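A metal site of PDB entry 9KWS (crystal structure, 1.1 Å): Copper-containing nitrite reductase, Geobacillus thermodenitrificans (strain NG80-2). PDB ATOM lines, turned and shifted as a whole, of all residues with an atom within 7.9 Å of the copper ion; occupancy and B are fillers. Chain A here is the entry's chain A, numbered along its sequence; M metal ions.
A ring nitrogen (NE2) of His 95 sits close to the backbone carbonyl oxygen of Val 93 (3.4 Å). NE2 of His 95 sits at hydrogen-bond distance from OD2 of Asp 90, 2.8 Å away. N of Val 113 sits at hydrogen-bond distance from O of His 95 (2.7 Å). OG1 of Thr 137 sits close to SG of Cys 135 (3.4 Å). SG of Cys 135 sits close to N of Ser 96. The backbone NH (N) of Met 148 lies close to the backbone carbonyl oxygen (O) of Trp 63 (3.3 Å).
Of the 27 residues printed, 4 come within 4 Å of the copper ion.
The copper ion is bound by ND1 of His 95 (2.0 Å), ND1 of His 143 (2.1 Å), SG of Cys 135 (2.2 Å) and SD of Met 148 (2.6 Å).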
ATOM      1  N   ALA A  47     -24.856  24.323 -32.618  1.00  0.00           N
ATOM      2  CA  ALA A  47     -25.149  23.365 -31.551  1.00  0.00           C
ATOM      3  C   ALA A  47     -25.763  22.153 -32.229  1.00  0.00           C
ATOM      4  O   ALA A  47     -26.701  22.306 -33.013  1.00  0.00           O
ATOM      5  CB  ALA A  47     -26.118  23.943 -30.527  1.00  0.00           C
ATOM      6  N   TRP A  63     -24.021  16.308 -26.779  1.00  0.00           N
ATOM      7  CA  TRP A  63     -24.466  17.657 -27.109  1.00  0.00           C
ATOM      8  C   TRP A  63     -23.208  18.456 -27.374  1.00  0.00           C
ATOM      9  O   TRP A  63     -22.304  18.474 -26.525  1.00  0.00           O
ATOM     10  CB  TRP A  63     -25.250  18.259 -25.958  1.00  0.00           C
ATOM     11  CG  TRP A  63     -26.474  17.516 -25.501  1.00  0.00           C
ATOM     12  CD1 TRP A  63     -26.938  16.303 -25.901  1.00  0.00           C
ATOM     13  CD2 TRP A  63     -27.406  17.988 -24.531  1.00  0.00           C
ATOM     14  NE1 TRP A  63     -28.099  15.987 -25.230  1.00  0.00           N
ATOM     15  CE2 TRP A  63     -28.404  17.020 -24.382  1.00  0.00           C
ATOM     16  CE3 TRP A  63     -27.473  19.153 -23.753  1.00  0.00           C
ATOM     17  CZ2 TRP A  63     -29.472  17.173 -23.494  1.00  0.00           C
ATOM     18  CZ3 TRP A  63     -28.517  19.285 -22.864  1.00  0.00           C
ATOM     19  CH2 TRP A  63     -29.509  18.308 -22.743  1.00  0.00           C
ATOM     20  N   THR A  64     -23.107  19.070 -28.558  1.00  0.00           N
ATOM     21  CA  THR A  64     -21.828  19.602 -28.987  1.00  0.00           C
ATOM     22  C   THR A  64     -21.965  20.954 -29.662  1.00  0.00           C
ATOM     23  O   THR A  64     -23.027  21.319 -30.177  1.00  0.00           O
ATOM     24  CB  THR A  64     -21.108  18.695 -30.006  1.00  0.00           C
ATOM     25  OG1 THR A  64     -21.739  18.786 -31.296  1.00  0.00           O
ATOM     26  CG2 THR A  64     -21.067  17.244 -29.543  1.00  0.00           C
ATOM     27  N   PHE A  65     -20.841  21.650 -29.716  1.00  0.00           N
ATOM     28  CA  PHE A  65     -20.606  22.681 -30.711  1.00  0.00           C
ATOM     29  C   PHE A  65     -19.911  22.040 -31.910  1.00  0.00           C
ATOM     30  O   PHE A  65     -18.829  21.454 -31.769  1.00  0.00           O
ATOM     31  CB  PHE A  65     -19.755  23.812 -30.129  1.00  0.00           C
ATOM     32  CG  PHE A  65     -20.425  24.551 -29.000  1.00  0.00           C
ATOM     33  CD1 PHE A  65     -21.487  25.418 -29.243  1.00  0.00           C
ATOM     34  CD2 PHE A  65     -20.026  24.343 -27.686  1.00  0.00           C
ATOM     35  CE1 PHE A  65     -22.083  26.094 -28.206  1.00  0.00           C
ATOM     36  CE2 PHE A  65     -20.632  25.040 -26.648  1.00  0.00           C
ATOM     37  CZ  PHE A  65     -21.657  25.913 -26.907  1.00  0.00           C
ATOM     38  N   LEU A  86     -24.613  31.569 -33.190  1.00  0.00           N
ATOM     39  CA  LEU A  86     -24.908  30.174 -32.892  1.00  0.00           C
ATOM     40  C   LEU A  86     -26.120  29.748 -33.710  1.00  0.00           C
ATOM     41  O   LEU A  86     -27.185  30.360 -33.610  1.00  0.00           O
ATOM     42  CB  LEU A  86     -25.211  29.973 -31.404  1.00  0.00           C
ATOM     43  CG  LEU A  86     -25.423  28.516 -30.981  1.00  0.00           C
ATOM     44  CD1 LEU A  86     -24.181  27.660 -31.199  1.00  0.00           C
ATOM     45  CD2 LEU A  86     -25.852  28.456 -29.513  1.00  0.00           C
ATOM     46  N   ASN A  88     -28.592  26.733 -33.944  1.00  0.00           N
ATOM     47  CA  ASN A  88     -29.007  25.599 -33.134  1.00  0.00           C
ATOM     48  C   ASN A  88     -29.647  24.545 -34.021  1.00  0.00           C
ATOM     49  O   ASN A  88     -30.771  24.732 -34.489  1.00  0.00           O
ATOM     50  CB  ASN A  88     -29.942  26.020 -32.008  1.00  0.00           C
ATOM     51  CG  ASN A  88     -30.231  24.881 -31.073  1.00  0.00           C
ATOM     52  OD1 ASN A  88     -29.711  23.779 -31.252  1.00  0.00           O
ATOM     53  ND2 ASN A  88     -31.037  25.139 -30.059  1.00  0.00           N
ATOM     54  N   ASP A  90     -30.105  21.398 -32.846  1.00  0.00           N
ATOM     55  CA  ASP A  90     -30.784  20.438 -31.988  1.00  0.00           C
ATOM     56  C   ASP A  90     -32.279  20.533 -32.266  1.00  0.00           C
ATOM     57  O   ASP A  90     -32.833  21.642 -32.291  1.00  0.00           O
ATOM     58  CB  ASP A  90     -30.484  20.819 -30.538  1.00  0.00           C
ATOM     59  CG  ASP A  90     -30.964  19.787 -29.507  1.00  0.00           C
ATOM     60  OD1 ASP A  90     -32.104  19.269 -29.646  1.00  0.00           O
ATOM     61  OD2 ASP A  90     -30.226  19.545 -28.520  1.00  0.00           O
ATOM     62  N   VAL A  93     -33.863  20.942 -27.927  1.00  0.00           N
ATOM     63  CA  VAL A  93     -33.260  21.601 -26.765  1.00  0.00           C
ATOM     64  C   VAL A  93     -32.681  22.952 -27.173  1.00  0.00           C
ATOM     65  O   VAL A  93     -31.913  23.009 -28.140  1.00  0.00           O
ATOM     66  CB  VAL A  93     -32.185  20.726 -26.098  1.00  0.00           C
ATOM     67  CG1 VAL A  93     -31.754  21.355 -24.790  1.00  0.00           C
ATOM     68  CG2 VAL A  93     -32.673  19.324 -25.858  1.00  0.00           C
ATOM     69  N   PRO A  94     -33.007  24.032 -26.464  1.00  0.00           N
ATOM     70  CA  PRO A  94     -32.295  25.305 -26.678  1.00  0.00           C
ATOM     71  C   PRO A  94     -30.842  25.209 -26.225  1.00  0.00           C
ATOM     72  O   PRO A  94     -30.511  24.437 -25.339  1.00  0.00           O
ATOM     73  CB  PRO A  94     -33.074  26.294 -25.774  1.00  0.00           C
ATOM     74  CG  PRO A  94     -34.406  25.626 -25.569  1.00  0.00           C
ATOM     75  CD  PRO A  94     -34.003  24.182 -25.388  1.00  0.00           C
ATOM     76  N   HIS A  95     -29.999  26.048 -26.826  1.00  0.00           N
ATOM     77  CA  HIS A  95     -28.584  26.124 -26.471  1.00  0.00           C
ATOM     78  C   HIS A  95     -28.124  27.567 -26.526  1.00  0.00           C
ATOM     79  O   HIS A  95     -28.809  28.440 -27.058  1.00  0.00           O
ATOM     80  CB  HIS A  95     -27.731  25.240 -27.395  1.00  0.00           C
ATOM     81  CG  HIS A  95     -28.062  23.792 -27.280  1.00  0.00           C
ATOM     82  ND1 HIS A  95     -27.764  23.047 -26.162  1.00  0.00           N
ATOM     83  CD2 HIS A  95     -28.703  22.967 -28.136  1.00  0.00           C
ATOM     84  CE1 HIS A  95     -28.210  21.817 -26.337  1.00  0.00           C
ATOM     85  NE2 HIS A  95     -28.784  21.745 -27.528  1.00  0.00           N
ATOM     86  N   SER A  96     -26.939  27.813 -25.975  1.00  0.00           N
ATOM     87  CA  SER A  96     -26.414  29.164 -25.857  1.00  0.00           C
ATOM     88  C   SER A  96     -24.889  29.083 -25.825  1.00  0.00           C
ATOM     89  O   SER A  96     -24.301  28.006 -25.911  1.00  0.00           O
ATOM     90  CB  SER A  96     -26.938  29.844 -24.592  1.00  0.00           C
ATOM     91  OG  SER A  96     -26.574  29.102 -23.440  1.00  0.00           O
ATOM     92  N   MET A  97     -24.259  30.245 -25.696  1.00  0.00           N
ATOM     93  CA  MET A  97     -22.804  30.359 -25.626  1.00  0.00           C
ATOM     94  C   MET A  97     -22.355  31.349 -24.574  1.00  0.00           C
ATOM     95  O   MET A  97     -22.780  32.511 -24.590  1.00  0.00           O
ATOM     96  CB  MET A  97     -22.210  30.747 -26.976  1.00  0.00           C
ATOM     97  CG  MET A  97     -20.704  30.925 -26.970  1.00  0.00           C
ATOM     98  SD  MET A  97     -19.725  29.535 -26.505  1.00  0.00           S
ATOM     99  CE  MET A  97     -19.637  28.724 -28.139  1.00  0.00           C
ATOM    100  N   ASP A 112     -30.511  32.022 -24.743  1.00  0.00           N
ATOM    101  CA  ASP A 112     -30.821  30.824 -25.481  1.00  0.00           C
ATOM    102  C   ASP A 112     -31.194  31.106 -26.932  1.00  0.00           C
ATOM    103  O   ASP A 112     -31.830  32.118 -27.253  1.00  0.00           O
ATOM    104  CB  ASP A 112     -31.956  30.057 -24.793  1.00  0.00           C
ATOM    105  CG  ASP A 112     -31.545  29.477 -23.449  1.00  0.00           C
ATOM    106  OD1 ASP A 112     -30.335  29.328 -23.190  1.00  0.00           O
ATOM    107  OD2 ASP A 112     -32.442  29.176 -22.631  1.00  0.00           O
ATOM    108  N   VAL A 113     -30.800  30.180 -27.797  1.00  0.00           N
ATOM    109  CA  VAL A 113     -31.181  30.111 -29.197  1.00  0.00           C
ATOM    110  C   VAL A 113     -32.045  28.869 -29.326  1.00  0.00           C
ATOM    111  O   VAL A 113     -31.620  27.766 -28.954  1.00  0.00           O
ATOM    112  CB  VAL A 113     -29.949  30.042 -30.101  1.00  0.00           C
ATOM    113  CG1 VAL A 113     -30.355  29.906 -31.558  1.00  0.00           C
ATOM    114  CG2 VAL A 113     -29.060  31.265 -29.885  1.00  0.00           C
ATOM    115  N   HIS A 134     -18.529  27.524 -23.120  1.00  0.00           N
ATOM    116  CA  HIS A 134     -19.478  26.446 -22.913  1.00  0.00           C
ATOM    117  C   HIS A 134     -20.888  26.950 -23.139  1.00  0.00           C
ATOM    118  O   HIS A 134     -21.160  28.137 -23.099  1.00  0.00           O
ATOM    119  CB  HIS A 134     -19.351  25.852 -21.495  1.00  0.00           C
ATOM    120  CG  HIS A 134     -19.554  26.854 -20.400  1.00  0.00           C
ATOM    121  ND1 HIS A 134     -20.795  27.156 -19.877  1.00  0.00           N
ATOM    122  CD2 HIS A 134     -18.669  27.609 -19.695  1.00  0.00           C
ATOM    123  CE1 HIS A 134     -20.659  28.040 -18.899  1.00  0.00           C
ATOM    124  NE2 HIS A 134     -19.383  28.338 -18.776  1.00  0.00           N
ATOM    125  N   CYS A 135     -21.810  26.010 -23.316  1.00  0.00           N
ATOM    126  CA  CYS A 135     -23.212  26.371 -23.331  1.00  0.00           C
ATOM    127  C   CYS A 135     -23.633  26.854 -21.946  1.00  0.00           C
ATOM    128  O   CYS A 135     -23.204  26.312 -20.923  1.00  0.00           O
ATOM    129  CB  CYS A 135     -24.036  25.168 -23.744  1.00  0.00           C
ATOM    130  SG  CYS A 135     -25.823  25.487 -23.803  1.00  0.00           S
ATOM    131  N   GLY A 136     -24.464  27.886 -21.928  1.00  0.00           N
ATOM    132  CA  GLY A 136     -24.948  28.488 -20.703  1.00  0.00           C
ATOM    133  C   GLY A 136     -26.424  28.300 -20.442  1.00  0.00           C
ATOM    134  O   GLY A 136     -27.017  29.083 -19.699  1.00  0.00           O
ATOM    135  N   THR A 137     -27.045  27.280 -21.025  1.00  0.00           N
ATOM    136  CA  THR A 137     -28.477  27.035 -20.896  1.00  0.00           C
ATOM    137  C   THR A 137     -28.744  26.233 -19.629  1.00  0.00           C
ATOM    138  O   THR A 137     -28.042  25.270 -19.311  1.00  0.00           O
ATOM    139  CB  THR A 137     -28.969  26.311 -22.142  1.00  0.00           C
ATOM    140  OG1 THR A 137     -28.727  27.154 -23.288  1.00  0.00           O
ATOM    141  CG2 THR A 137     -30.442  25.972 -22.077  1.00  0.00           C
ATOM    142  N   LYS A 138     -29.792  26.630 -18.905  1.00  0.00           N
ATOM    143  CA  LYS A 138     -30.120  25.954 -17.650  1.00  0.00           C
ATOM    144  C   LYS A 138     -30.728  24.590 -17.953  1.00  0.00           C
ATOM    145  O   LYS A 138     -31.541  24.461 -18.864  1.00  0.00           O
ATOM    146  CB  LYS A 138     -31.134  26.805 -16.867  1.00  0.00           C
ATOM    147  CG  LYS A 138     -31.914  26.039 -15.816  1.00  0.00           C
ATOM    148  CD  LYS A 138     -32.452  26.952 -14.718  1.00  0.00           C
ATOM    149  CE  LYS A 138     -32.804  26.121 -13.491  1.00  0.00           C
ATOM    150  NZ  LYS A 138     -32.182  24.755 -13.570  1.00  0.00           N
ATOM    151  N   PRO A 139     -30.348  23.532 -17.208  1.00  0.00           N
ATOM    152  CA  PRO A 139     -29.300  23.487 -16.169  1.00  0.00           C
ATOM    153  C   PRO A 139     -27.921  23.416 -16.815  1.00  0.00           C
ATOM    154  O   PRO A 139     -27.643  22.531 -17.622  1.00  0.00           O
ATOM    155  CB  PRO A 139     -29.587  22.185 -15.416  1.00  0.00           C
ATOM    156  CG  PRO A 139     -30.806  21.608 -16.002  1.00  0.00           C
ATOM    157  CD  PRO A 139     -31.031  22.232 -17.333  1.00  0.00           C
ATOM    158  N   VAL A 140     -27.051  24.364 -16.458  1.00  0.00           N
ATOM    159  CA  VAL A 140     -25.757  24.453 -17.122  1.00  0.00           C
ATOM    160  C   VAL A 140     -24.948  23.185 -16.926  1.00  0.00           C
ATOM    161  O   VAL A 140     -24.279  22.729 -17.849  1.00  0.00           O
ATOM    162  CB  VAL A 140     -25.017  25.722 -16.651  1.00  0.00           C
ATOM    163  CG1 VAL A 140     -23.611  25.763 -17.201  1.00  0.00           C
ATOM    164  CG2 VAL A 140     -25.787  26.961 -17.066  1.00  0.00           C
ATOM    165  N   GLN A 142     -25.960  20.185 -16.948  1.00  0.00           N
ATOM    166  CA  GLN A 142     -26.397  19.206 -17.947  1.00  0.00           C
ATOM    167  C   GLN A 142     -25.787  19.499 -19.315  1.00  0.00           C
ATOM    168  O   GLN A 142     -25.326  18.583 -20.020  1.00  0.00           O
ATOM    169  CB  GLN A 142     -27.926  19.216 -18.031  1.00  0.00           C
ATOM    170  CG  GLN A 142     -28.488  18.170 -18.958  1.00  0.00           C
ATOM    171  CD  GLN A 142     -29.997  18.129 -18.936  1.00  0.00           C
ATOM    172  OE1 GLN A 142     -30.650  19.080 -18.509  1.00  0.00           O
ATOM    173  NE2 GLN A 142     -30.554  17.024 -19.390  1.00  0.00           N
ATOM    174  N   HIS A 143     -25.795  20.762 -19.719  1.00  0.00           N
ATOM    175  CA  HIS A 143     -25.266  21.104 -21.035  1.00  0.00           C
ATOM    176  C   HIS A 143     -23.753  20.913 -21.097  1.00  0.00           C
ATOM    177  O   HIS A 143     -23.225  20.342 -22.076  1.00  0.00           O
ATOM    178  CB  HIS A 143     -25.707  22.511 -21.394  1.00  0.00           C
ATOM    179  CG  HIS A 143     -27.175  22.592 -21.695  1.00  0.00           C
ATOM    180  ND1 HIS A 143     -27.654  22.715 -22.975  1.00  0.00           N
ATOM    181  CD2 HIS A 143     -28.257  22.534 -20.889  1.00  0.00           C
ATOM    182  CE1 HIS A 143     -28.974  22.755 -22.940  1.00  0.00           C
ATOM    183  NE2 HIS A 143     -29.367  22.642 -21.694  1.00  0.00           N
ATOM    184  N   ILE A 144     -23.034  21.339 -20.048  1.00  0.00           N
ATOM    185  CA  ILE A 144     -21.590  21.098 -20.043  1.00  0.00           C
ATOM    186  C   ILE A 144     -21.313  19.602 -20.022  1.00  0.00           C
ATOM    187  O   ILE A 144     -20.518  19.087 -20.824  1.00  0.00           O
ATOM    188  CB  ILE A 144     -20.904  21.819 -18.874  1.00  0.00           C
ATOM    189  CG1 ILE A 144     -21.080  23.339 -18.958  1.00  0.00           C
ATOM    190  CG2 ILE A 144     -19.418  21.439 -18.868  1.00  0.00           C
ATOM    191  CD1 ILE A 144     -20.485  24.085 -17.784  1.00  0.00           C
ATOM    192  N   ASN A 146     -22.897  17.042 -20.976  1.00  0.00           N
ATOM    193  CA  ASN A 146     -23.205  16.324 -22.208  1.00  0.00           C
ATOM    194  C   ASN A 146     -22.273  16.659 -23.363  1.00  0.00           C
ATOM    195  O   ASN A 146     -22.374  16.009 -24.413  1.00  0.00           O
ATOM    196  CB  ASN A 146     -24.654  16.543 -22.615  1.00  0.00           C
ATOM    197  CG  ASN A 146     -25.637  15.677 -21.841  1.00  0.00           C
ATOM    198  OD1 ASN A 146     -25.344  14.538 -21.473  1.00  0.00           O
ATOM    199  ND2 ASN A 146     -26.829  16.217 -21.614  1.00  0.00           N
ATOM    200  N   GLY A 147     -21.362  17.632 -23.199  1.00  0.00           N
ATOM    201  CA  GLY A 147     -20.311  17.874 -24.158  1.00  0.00           C
ATOM    202  C   GLY A 147     -20.115  19.298 -24.627  1.00  0.00           C
ATOM    203  O   GLY A 147     -19.214  19.519 -25.438  1.00  0.00           O
ATOM    204  N   MET A 148     -20.890  20.270 -24.135  1.00  0.00           N
ATOM    205  CA  MET A 148     -20.885  21.626 -24.707  1.00  0.00           C
ATOM    206  C   MET A 148     -19.878  22.520 -23.981  1.00  0.00           C
ATOM    207  O   MET A 148     -20.224  23.415 -23.213  1.00  0.00           O
ATOM    208  CB  MET A 148     -22.289  22.223 -24.651  1.00  0.00           C
ATOM    209  CG  MET A 148     -23.311  21.323 -25.325  1.00  0.00           C
ATOM    210  SD  MET A 148     -24.880  22.074 -25.731  1.00  0.00           S
ATOM    211  CE  MET A 148     -24.391  23.039 -27.124  1.00  0.00           C
HETATM  212 CU    CU M   1     -26.655  23.595 -24.545  1.00  0.00          CU
